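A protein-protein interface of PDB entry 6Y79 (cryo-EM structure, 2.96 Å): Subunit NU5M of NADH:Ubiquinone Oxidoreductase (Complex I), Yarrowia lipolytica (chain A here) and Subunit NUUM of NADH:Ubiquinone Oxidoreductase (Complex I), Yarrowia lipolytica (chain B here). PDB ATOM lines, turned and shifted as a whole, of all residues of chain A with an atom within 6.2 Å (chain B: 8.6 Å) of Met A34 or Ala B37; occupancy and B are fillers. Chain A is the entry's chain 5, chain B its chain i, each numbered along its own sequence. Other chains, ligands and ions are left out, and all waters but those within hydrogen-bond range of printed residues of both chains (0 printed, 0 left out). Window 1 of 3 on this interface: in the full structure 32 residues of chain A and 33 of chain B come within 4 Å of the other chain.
The backbone carbonyl oxygen of Gly B30 sits at hydrogen-bond distance from the side-chain hydroxyl of Thr B34 (2.4 Å).
Among the printed residues, pairs that only touch across the chains: Ile A14 with Ala B37 (3.7 Å), Ile A14 with Leu B40 (3.9 Å), Ile A14 with Ala B41 (3.8 Å), Phe A18 with Ile B36 (3.6 Å), Phe A18 with Ala B37 (3.6 Å), Leu A26 with Trp B26 (3.2 Å), Leu A26 with Asn B29 (3.3 Å), Leu A26 with Gly B30 (3.7 Å), Leu A26 with Ala B33 (3.8 Å), Val A29 with Trp B26 (3.8 Å), Phe A30 with Trp B26 (3.6 Å), Phe A30 with Gly B30 (3.5 Å), Phe A30 with Ala B33 (3.99 Å), Met A34 with Ala B33 (3.6 Å) and Met A34 with Ala B37 (3.6 Å).
Thr A32 touches none of the printed residues of chain B. Of chain B, only Ala B33 (3.6 Å) and Ala B37 (3.6 Å) come within 4 Å of Met A34. Of the printed residues of chain A, Trp B26 touches Leu A26 (3.2 Å), Val A29 (3.8 Å) and Phe A30 (3.6 Å). Of the printed residues of chain A, Asn B29 touches Leu A26. Of the printed residues of chain A, Gly B30 touches Leu A26 (3.7 Å) and Phe A30 (3.5 Å). Thr B34 touches none of the printed residues of chain A. Of chain A, only Ile A14 (3.7 Å), Phe A18 (3.6 Å) and Met A34 (3.6 Å) come within 4 Å of Ala B37. Of the printed residues of chain A, Ala B41 touches Ile A14. The nearest residue of chain B that does not touch Met A34 is Thr B34 (4.5 Å). The nearest residue of chain A that does not touch Ala B37 is Leu A38 (4.8 Å). The nearest printed residue of chain A that does not touch Asn B29 is Phe A30 (5.3 Å).
Of the 17 printed residues of chain B, 8 touch a printed residue of chain A. Printed residues of chain B that touch a printed residue of chain A: Trp B26, Asn B29, Gly B30, Ala B33, Ile B36, Ala B37, Leu B40 and Ala B41. Among the printed residues, no Asp or Glu carboxylate lies within 4 Å of a Lys or Arg side-chain nitrogen of the other chain.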
ATOM      1  N   ILE A  14       6.604 -19.067  15.761  1.00  0.00           N
ATOM      2  CA  ILE A  14       6.372 -19.182  17.198  1.00  0.00           C
ATOM      3  C   ILE A  14       6.009 -20.615  17.550  1.00  0.00           C
ATOM      4  O   ILE A  14       6.592 -21.226  18.460  1.00  0.00           O
ATOM      5  CB  ILE A  14       5.278 -18.189  17.629  1.00  0.00           C
ATOM      6  CG1 ILE A  14       5.807 -16.759  17.563  1.00  0.00           C
ATOM      7  CG2 ILE A  14       4.790 -18.485  19.010  1.00  0.00           C
ATOM      8  CD1 ILE A  14       4.724 -15.727  17.532  1.00  0.00           C
ATOM      9  N   SER A  15       5.098 -21.197  16.768  1.00  0.00           N
ATOM     10  CA  SER A  15       4.629 -22.570  16.912  1.00  0.00           C
ATOM     11  C   SER A  15       5.722 -23.614  16.723  1.00  0.00           C
ATOM     12  O   SER A  15       5.518 -24.766  17.110  1.00  0.00           O
ATOM     13  CB  SER A  15       3.501 -22.816  15.916  1.00  0.00           C
ATOM     14  OG  SER A  15       3.026 -24.139  15.993  1.00  0.00           O
ATOM     15  N   PHE A  18       8.941 -22.359  19.994  1.00  0.00           N
ATOM     16  CA  PHE A  18       8.610 -22.528  21.405  1.00  0.00           C
ATOM     17  C   PHE A  18       8.482 -23.986  21.873  1.00  0.00           C
ATOM     18  O   PHE A  18       8.817 -24.249  23.034  1.00  0.00           O
ATOM     19  CB  PHE A  18       7.350 -21.728  21.750  1.00  0.00           C
ATOM     20  CG  PHE A  18       7.567 -20.236  21.792  1.00  0.00           C
ATOM     21  CD1 PHE A  18       8.836 -19.684  21.645  1.00  0.00           C
ATOM     22  CD2 PHE A  18       6.504 -19.388  22.008  1.00  0.00           C
ATOM     23  CE1 PHE A  18       9.027 -18.327  21.681  1.00  0.00           C
ATOM     24  CE2 PHE A  18       6.692 -18.025  22.049  1.00  0.00           C
ATOM     25  CZ  PHE A  18       7.955 -17.495  21.884  1.00  0.00           C
ATOM     26  N   PRO A  19       7.986 -24.951  21.076  1.00  0.00           N
ATOM     27  CA  PRO A  19       8.092 -26.352  21.519  1.00  0.00           C
ATOM     28  C   PRO A  19       9.506 -26.878  21.679  1.00  0.00           C
ATOM     29  O   PRO A  19       9.704 -27.847  22.416  1.00  0.00           O
ATOM     30  CB  PRO A  19       7.355 -27.116  20.419  1.00  0.00           C
ATOM     31  CG  PRO A  19       6.344 -26.205  19.977  1.00  0.00           C
ATOM     32  CD  PRO A  19       6.948 -24.846  20.028  1.00  0.00           C
ATOM     33  N   LEU A  26       7.259 -27.100  29.331  1.00  0.00           N
ATOM     34  CA  LEU A  26       5.816 -27.079  29.119  1.00  0.00           C
ATOM     35  C   LEU A  26       5.199 -28.466  29.025  1.00  0.00           C
ATOM     36  O   LEU A  26       4.113 -28.683  29.558  1.00  0.00           O
ATOM     37  CB  LEU A  26       5.468 -26.303  27.849  1.00  0.00           C
ATOM     38  CG  LEU A  26       5.820 -24.826  27.762  1.00  0.00           C
ATOM     39  CD1 LEU A  26       5.681 -24.359  26.331  1.00  0.00           C
ATOM     40  CD2 LEU A  26       4.919 -24.042  28.652  1.00  0.00           C
ATOM     41  N   VAL A  29       1.266 -32.420  26.851  1.00  0.00           N
ATOM     42  CA  VAL A  29      -0.157 -32.104  26.908  1.00  0.00           C
ATOM     43  C   VAL A  29      -0.391 -30.605  26.751  1.00  0.00           C
ATOM     44  O   VAL A  29      -1.423 -30.185  26.217  1.00  0.00           O
ATOM     45  CB  VAL A  29      -0.776 -32.680  28.202  1.00  0.00           C
ATOM     46  CG1 VAL A  29      -0.205 -32.023  29.439  1.00  0.00           C
ATOM     47  CG2 VAL A  29      -2.295 -32.586  28.180  1.00  0.00           C
ATOM     48  N   PHE A  30       0.575 -29.772  27.135  1.00  0.00           N
ATOM     49  CA  PHE A  30       0.391 -28.360  26.840  1.00  0.00           C
ATOM     50  C   PHE A  30       0.779 -28.031  25.411  1.00  0.00           C
ATOM     51  O   PHE A  30       0.045 -27.306  24.728  1.00  0.00           O
ATOM     52  CB  PHE A  30       1.189 -27.463  27.774  1.00  0.00           C
ATOM     53  CG  PHE A  30       1.015 -26.011  27.449  1.00  0.00           C
ATOM     54  CD1 PHE A  30      -0.192 -25.388  27.702  1.00  0.00           C
ATOM     55  CD2 PHE A  30       2.021 -25.287  26.829  1.00  0.00           C
ATOM     56  CE1 PHE A  30      -0.384 -24.063  27.382  1.00  0.00           C
ATOM     57  CE2 PHE A  30       1.831 -23.965  26.504  1.00  0.00           C
ATOM     58  CZ  PHE A  30       0.622 -23.355  26.769  1.00  0.00           C
ATOM     59  N   VAL A  31       1.947 -28.514  24.966  1.00  0.00           N
ATOM     60  CA  VAL A  31       2.521 -28.089  23.693  1.00  0.00           C
ATOM     61  C   VAL A  31       1.675 -28.540  22.519  1.00  0.00           C
ATOM     62  O   VAL A  31       1.563 -27.815  21.531  1.00  0.00           O
ATOM     63  CB  VAL A  31       3.981 -28.586  23.632  1.00  0.00           C
ATOM     64  CG1 VAL A  31       4.536 -28.636  22.230  1.00  0.00           C
ATOM     65  CG2 VAL A  31       4.850 -27.659  24.445  1.00  0.00           C
ATOM     66  N   THR A  32       1.005 -29.682  22.637  1.00  0.00           N
ATOM     67  CA  THR A  32       0.041 -30.162  21.651  1.00  0.00           C
ATOM     68  C   THR A  32      -1.096 -29.189  21.373  1.00  0.00           C
ATOM     69  O   THR A  32      -1.328 -28.768  20.222  1.00  0.00           O
ATOM     70  CB  THR A  32      -0.558 -31.463  22.170  1.00  0.00           C
ATOM     71  OG1 THR A  32       0.496 -32.411  22.380  1.00  0.00           O
ATOM     72  CG2 THR A  32      -1.498 -32.010  21.181  1.00  0.00           C
ATOM     73  N   ARG A  33      -1.787 -28.817  22.461  1.00  0.00           N
ATOM     74  CA  ARG A  33      -2.878 -27.856  22.381  1.00  0.00           C
ATOM     75  C   ARG A  33      -2.380 -26.492  21.930  1.00  0.00           C
ATOM     76  O   ARG A  33      -3.056 -25.825  21.145  1.00  0.00           O
ATOM     77  CB  ARG A  33      -3.599 -27.736  23.725  1.00  0.00           C
ATOM     78  CG  ARG A  33      -4.031 -29.052  24.380  1.00  0.00           C
ATOM     79  CD  ARG A  33      -4.801 -29.939  23.405  1.00  0.00           C
ATOM     80  NE  ARG A  33      -5.599 -30.969  24.068  1.00  0.00           N
ATOM     81  CZ  ARG A  33      -5.116 -32.122  24.520  1.00  0.00           C
ATOM     82  NH1 ARG A  33      -3.826 -32.401  24.404  1.00  0.00           N
ATOM     83  NH2 ARG A  33      -5.927 -32.996  25.094  1.00  0.00           N
ATOM     84  N   MET A  34      -1.168 -26.105  22.333  1.00  0.00           N
ATOM     85  CA  MET A  34      -0.642 -24.798  21.948  1.00  0.00           C
ATOM     86  C   MET A  34      -0.295 -24.741  20.465  1.00  0.00           C
ATOM     87  O   MET A  34      -0.661 -23.784  19.770  1.00  0.00           O
ATOM     88  CB  MET A  34       0.583 -24.442  22.783  1.00  0.00           C
ATOM     89  CG  MET A  34       1.117 -23.091  22.413  1.00  0.00           C
ATOM     90  SD  MET A  34       2.511 -22.528  23.374  1.00  0.00           S
ATOM     91  CE  MET A  34       2.452 -20.807  22.940  1.00  0.00           C
ATOM     92  N   THR A  35       0.446 -25.746  19.977  1.00  0.00           N
ATOM     93  CA  THR A  35       0.875 -25.802  18.582  1.00  0.00           C
ATOM     94  C   THR A  35      -0.319 -25.825  17.645  1.00  0.00           C
ATOM     95  O   THR A  35      -0.387 -25.037  16.684  1.00  0.00           O
ATOM     96  CB  THR A  35       1.752 -27.039  18.359  1.00  0.00           C
ATOM     97  OG1 THR A  35       2.965 -26.933  19.107  1.00  0.00           O
ATOM     98  CG2 THR A  35       2.098 -27.205  16.904  1.00  0.00           C
ATOM     99  N   SER A  36      -1.307 -26.669  17.960  1.00  0.00           N
ATOM    100  CA  SER A  36      -2.537 -26.727  17.187  1.00  0.00           C
ATOM    101  C   SER A  36      -3.345 -25.441  17.263  1.00  0.00           C
ATOM    102  O   SER A  36      -3.793 -24.982  16.213  1.00  0.00           O
ATOM    103  CB  SER A  36      -3.366 -27.934  17.643  1.00  0.00           C
ATOM    104  OG  SER A  36      -2.692 -29.123  17.377  1.00  0.00           O
ATOM    105  N   THR A  37      -3.507 -24.874  18.478  1.00  0.00           N
ATOM    106  CA  THR A  37      -4.175 -23.587  18.685  1.00  0.00           C
ATOM    107  C   THR A  37      -3.599 -22.483  17.799  1.00  0.00           C
ATOM    108  O   THR A  37      -4.349 -21.741  17.138  1.00  0.00           O
ATOM    109  CB  THR A  37      -4.048 -23.177  20.151  1.00  0.00           C
ATOM    110  OG1 THR A  37      -4.624 -24.154  21.012  1.00  0.00           O
ATOM    111  CG2 THR A  37      -4.685 -21.812  20.429  1.00  0.00           C
ATOM    112  N   LEU A  38      -2.274 -22.413  17.716  1.00  0.00           N
ATOM    113  CA  LEU A  38      -1.634 -21.349  16.961  1.00  0.00           C
ATOM    114  C   LEU A  38      -1.785 -21.573  15.464  1.00  0.00           C
ATOM    115  O   LEU A  38      -1.993 -20.616  14.711  1.00  0.00           O
ATOM    116  CB  LEU A  38      -0.164 -21.246  17.372  1.00  0.00           C
ATOM    117  CG  LEU A  38       0.207 -20.258  18.482  1.00  0.00           C
ATOM    118  CD1 LEU A  38      -0.557 -20.469  19.798  1.00  0.00           C
ATOM    119  CD2 LEU A  38       1.667 -20.423  18.735  1.00  0.00           C
ATOM    120  N   ILE A  39      -1.716 -22.832  15.010  1.00  0.00           N
ATOM    121  CA  ILE A  39      -1.938 -23.077  13.582  1.00  0.00           C
ATOM    122  C   ILE A  39      -3.413 -22.864  13.207  1.00  0.00           C
ATOM    123  O   ILE A  39      -3.717 -22.434  12.083  1.00  0.00           O
ATOM    124  CB  ILE A  39      -1.417 -24.480  13.204  1.00  0.00           C
ATOM    125  CG1 ILE A  39       0.073 -24.606  13.527  1.00  0.00           C
ATOM    126  CG2 ILE A  39      -1.548 -24.750  11.729  1.00  0.00           C
ATOM    127  CD1 ILE A  39       0.966 -23.627  12.802  1.00  0.00           C
ATOM    128  N   TRP B  26       2.629 -27.458  34.436  1.00  0.00           N
ATOM    129  CA  TRP B  26       2.518 -27.157  33.017  1.00  0.00           C
ATOM    130  C   TRP B  26       1.438 -26.133  32.728  1.00  0.00           C
ATOM    131  O   TRP B  26       1.533 -25.427  31.718  1.00  0.00           O
ATOM    132  CB  TRP B  26       2.267 -28.430  32.211  1.00  0.00           C
ATOM    133  CG  TRP B  26       1.007 -29.150  32.500  1.00  0.00           C
ATOM    134  CD1 TRP B  26       0.825 -30.118  33.430  1.00  0.00           C
ATOM    135  CD2 TRP B  26      -0.244 -29.002  31.822  1.00  0.00           C
ATOM    136  NE1 TRP B  26      -0.464 -30.576  33.394  1.00  0.00           N
ATOM    137  CE2 TRP B  26      -1.143 -29.906  32.413  1.00  0.00           C
ATOM    138  CE3 TRP B  26      -0.696 -28.187  30.782  1.00  0.00           C
ATOM    139  CZ2 TRP B  26      -2.466 -30.022  31.997  1.00  0.00           C
ATOM    140  CZ3 TRP B  26      -2.010 -28.302  30.371  1.00  0.00           C
ATOM    141  CH2 TRP B  26      -2.878 -29.215  30.976  1.00  0.00           C
ATOM    142  N   ASN B  29       3.572 -22.777  33.678  1.00  0.00           N
ATOM    143  CA  ASN B  29       4.469 -22.428  32.584  1.00  0.00           C
ATOM    144  C   ASN B  29       3.702 -22.119  31.309  1.00  0.00           C
ATOM    145  O   ASN B  29       4.185 -21.350  30.463  1.00  0.00           O
ATOM    146  CB  ASN B  29       5.444 -23.565  32.328  1.00  0.00           C
ATOM    147  CG  ASN B  29       6.328 -23.838  33.501  1.00  0.00           C
ATOM    148  OD1 ASN B  29       6.678 -22.933  34.248  1.00  0.00           O
ATOM    149  ND2 ASN B  29       6.708 -25.092  33.672  1.00  0.00           N
ATOM    150  N   GLY B  30       2.524 -22.728  31.139  1.00  0.00           N
ATOM    151  CA  GLY B  30       1.727 -22.460  29.961  1.00  0.00           C
ATOM    152  C   GLY B  30       1.231 -21.035  29.895  1.00  0.00           C
ATOM    153  O   GLY B  30       1.080 -20.477  28.807  1.00  0.00           O
ATOM    154  N   LEU B  31       0.980 -20.427  31.053  1.00  0.00           N
ATOM    155  CA  LEU B  31       0.619 -19.008  31.086  1.00  0.00           C
ATOM    156  C   LEU B  31       1.772 -18.113  30.619  1.00  0.00           C
ATOM    157  O   LEU B  31       1.549 -17.121  29.906  1.00  0.00           O
ATOM    158  CB  LEU B  31       0.140 -18.619  32.487  1.00  0.00           C
ATOM    159  CG  LEU B  31      -1.368 -18.739  32.785  1.00  0.00           C
ATOM    160  CD1 LEU B  31      -1.885 -20.201  32.914  1.00  0.00           C
ATOM    161  CD2 LEU B  31      -1.777 -17.893  34.000  1.00  0.00           C
ATOM    162  N   PHE B  32       3.016 -18.470  30.978  1.00  0.00           N
ATOM    163  CA  PHE B  32       4.184 -17.735  30.487  1.00  0.00           C
ATOM    164  C   PHE B  32       4.354 -17.891  28.983  1.00  0.00           C
ATOM    165  O   PHE B  32       4.658 -16.918  28.281  1.00  0.00           O
ATOM    166  CB  PHE B  32       5.458 -18.221  31.169  1.00  0.00           C
ATOM    167  CG  PHE B  32       5.557 -17.866  32.615  1.00  0.00           C
ATOM    168  CD1 PHE B  32       5.838 -16.573  33.007  1.00  0.00           C
ATOM    169  CD2 PHE B  32       5.406 -18.840  33.588  1.00  0.00           C
ATOM    170  CE1 PHE B  32       5.935 -16.251  34.344  1.00  0.00           C
ATOM    171  CE2 PHE B  32       5.502 -18.526  34.925  1.00  0.00           C
ATOM    172  CZ  PHE B  32       5.767 -17.234  35.304  1.00  0.00           C
ATOM    173  N   ALA B  33       4.200 -19.120  28.480  1.00  0.00           N
ATOM    174  CA  ALA B  33       4.333 -19.359  27.044  1.00  0.00           C
ATOM    175  C   ALA B  33       3.236 -18.651  26.259  1.00  0.00           C
ATOM    176  O   ALA B  33       3.494 -18.115  25.172  1.00  0.00           O
ATOM    177  CB  ALA B  33       4.317 -20.857  26.758  1.00  0.00           C
ATOM    178  N   THR B  34       2.019 -18.619  26.817  1.00  0.00           N
ATOM    179  CA  THR B  34       0.913 -17.851  26.260  1.00  0.00           C
ATOM    180  C   THR B  34       1.262 -16.377  26.143  1.00  0.00           C
ATOM    181  O   THR B  34       1.060 -15.768  25.080  1.00  0.00           O
ATOM    182  CB  THR B  34      -0.315 -18.018  27.150  1.00  0.00           C
ATOM    183  OG1 THR B  34      -0.546 -19.407  27.403  1.00  0.00           O
ATOM    184  CG2 THR B  34      -1.548 -17.393  26.506  1.00  0.00           C
ATOM    185  N   GLY B  35       1.802 -15.800  27.225  1.00  0.00           N
ATOM    186  CA  GLY B  35       2.135 -14.383  27.221  1.00  0.00           C
ATOM    187  C   GLY B  35       3.237 -14.033  26.242  1.00  0.00           C
ATOM    188  O   GLY B  35       3.132 -13.053  25.500  1.00  0.00           O
ATOM    189  N   ILE B  36       4.296 -14.850  26.207  1.00  0.00           N
ATOM    190  CA  ILE B  36       5.416 -14.588  25.305  1.00  0.00           C
ATOM    191  C   ILE B  36       4.990 -14.755  23.850  1.00  0.00           C
ATOM    192  O   ILE B  36       5.374 -13.953  22.990  1.00  0.00           O
ATOM    193  CB  ILE B  36       6.614 -15.489  25.656  1.00  0.00           C
ATOM    194  CG1 ILE B  36       7.111 -15.180  27.060  1.00  0.00           C
ATOM    195  CG2 ILE B  36       7.769 -15.269  24.701  1.00  0.00           C
ATOM    196  CD1 ILE B  36       8.165 -16.130  27.532  1.00  0.00           C
ATOM    197  N   ALA B  37       4.141 -15.749  23.562  1.00  0.00           N
ATOM    198  CA  ALA B  37       3.701 -15.976  22.191  1.00  0.00           C
ATOM    199  C   ALA B  37       2.820 -14.845  21.689  1.00  0.00           C
ATOM    200  O   ALA B  37       3.024 -14.346  20.574  1.00  0.00           O
ATOM    201  CB  ALA B  37       2.958 -17.301  22.091  1.00  0.00           C
ATOM    202  N   VAL B  38       1.852 -14.406  22.504  1.00  0.00           N
ATOM    203  CA  VAL B  38       0.981 -13.330  22.039  1.00  0.00           C
ATOM    204  C   VAL B  38       1.741 -12.005  21.988  1.00  0.00           C
ATOM    205  O   VAL B  38       1.542 -11.214  21.064  1.00  0.00           O
ATOM    206  CB  VAL B  38      -0.314 -13.247  22.877  1.00  0.00           C
ATOM    207  CG1 VAL B  38      -0.066 -12.826  24.309  1.00  0.00           C
ATOM    208  CG2 VAL B  38      -1.315 -12.308  22.228  1.00  0.00           C
ATOM    209  N   GLY B  39       2.693 -11.784  22.905  1.00  0.00           N
ATOM    210  CA  GLY B  39       3.458 -10.548  22.873  1.00  0.00           C
ATOM    211  C   GLY B  39       4.399 -10.476  21.690  1.00  0.00           C
ATOM    212  O   GLY B  39       4.518  -9.432  21.045  1.00  0.00           O
ATOM    213  N   LEU B  40       5.034 -11.600  21.353  1.00  0.00           N
ATOM    214  CA  LEU B  40       5.917 -11.638  20.197  1.00  0.00           C
ATOM    215  C   LEU B  40       5.136 -11.515  18.897  1.00  0.00           C
ATOM    216  O   LEU B  40       5.569 -10.807  17.982  1.00  0.00           O
ATOM    217  CB  LEU B  40       6.732 -12.925  20.217  1.00  0.00           C
ATOM    218  CG  LEU B  40       7.770 -13.054  19.110  1.00  0.00           C
ATOM    219  CD1 LEU B  40       8.797 -11.957  19.245  1.00  0.00           C
ATOM    220  CD2 LEU B  40       8.426 -14.416  19.164  1.00  0.00           C
ATOM    221  N   ALA B  41       3.973 -12.170  18.805  1.00  0.00           N
ATOM    222  CA  ALA B  41       3.163 -12.070  17.595  1.00  0.00           C
ATOM    223  C   ALA B  41       2.621 -10.657  17.405  1.00  0.00           C
ATOM    224  O   ALA B  41       2.677 -10.111  16.299  1.00  0.00           O
ATOM    225  CB  ALA B  41       2.026 -13.089  17.639  1.00  0.00           C
ATOM    226  N   LEU B  42       2.138 -10.033  18.489  1.00  0.00           N
ATOM    227  CA  LEU B  42       1.667  -8.649  18.443  1.00  0.00           C
ATOM    228  C   LEU B  42       2.788  -7.688  18.072  1.00  0.00           C
ATOM    229  O   LEU B  42       2.589  -6.760  17.276  1.00  0.00           O
ATOM    230  CB  LEU B  42       1.092  -8.250  19.803  1.00  0.00           C
ATOM    231  CG  LEU B  42      -0.287  -8.692  20.296  1.00  0.00           C
ATOM    232  CD1 LEU B  42      -0.425  -8.335  21.772  1.00  0.00           C
ATOM    233  CD2 LEU B  42      -1.422  -8.118  19.474  1.00  0.00           C
ATOM    234  N   TRP B  43       3.980  -7.906  18.623  1.00  0.00           N
ATOM    235  CA  TRP B  43       5.067  -6.965  18.409  1.00  0.00           C
ATOM    236  C   TRP B  43       5.639  -7.074  16.999  1.00  0.00           C
ATOM    237  O   TRP B  43       5.931  -6.049  16.369  1.00  0.00           O
ATOM    238  CB  TRP B  43       6.143  -7.191  19.463  1.00  0.00           C
ATOM    239  CG  TRP B  43       7.242  -6.244  19.324  1.00  0.00           C
ATOM    240  CD1 TRP B  43       7.201  -4.903  19.537  1.00  0.00           C
ATOM    241  CD2 TRP B  43       8.562  -6.548  18.899  1.00  0.00           C
ATOM    242  NE1 TRP B  43       8.428  -4.350  19.281  1.00  0.00           N
ATOM    243  CE2 TRP B  43       9.282  -5.344  18.886  1.00  0.00           C
ATOM    244  CE3 TRP B  43       9.209  -7.728  18.529  1.00  0.00           C
ATOM    245  CZ2 TRP B  43      10.617  -5.284  18.518  1.00  0.00           C
ATOM    246  CZ3 TRP B  43      10.533  -7.668  18.164  1.00  0.00           C
ATOM    247  CH2 TRP B  43      11.223  -6.455  18.160  1.00  0.00           C
ATOM    248  N   VAL B  44       5.794  -8.301  16.485  1.00  0.00           N
ATOM    249  CA  VAL B  44       6.198  -8.487  15.092  1.00  0.00           C
ATOM    250  C   VAL B  44       5.111  -7.978  14.153  1.00  0.00           C
ATOM    251  O   VAL B  44       5.414  -7.405  13.095  1.00  0.00           O
ATOM    252  CB  VAL B  44       6.547  -9.970  14.838  1.00  0.00           C
ATOM    253  CG1 VAL B  44       6.754 -10.263  13.364  1.00  0.00           C
ATOM    254  CG2 VAL B  44       7.799 -10.354  15.595  1.00  0.00           C
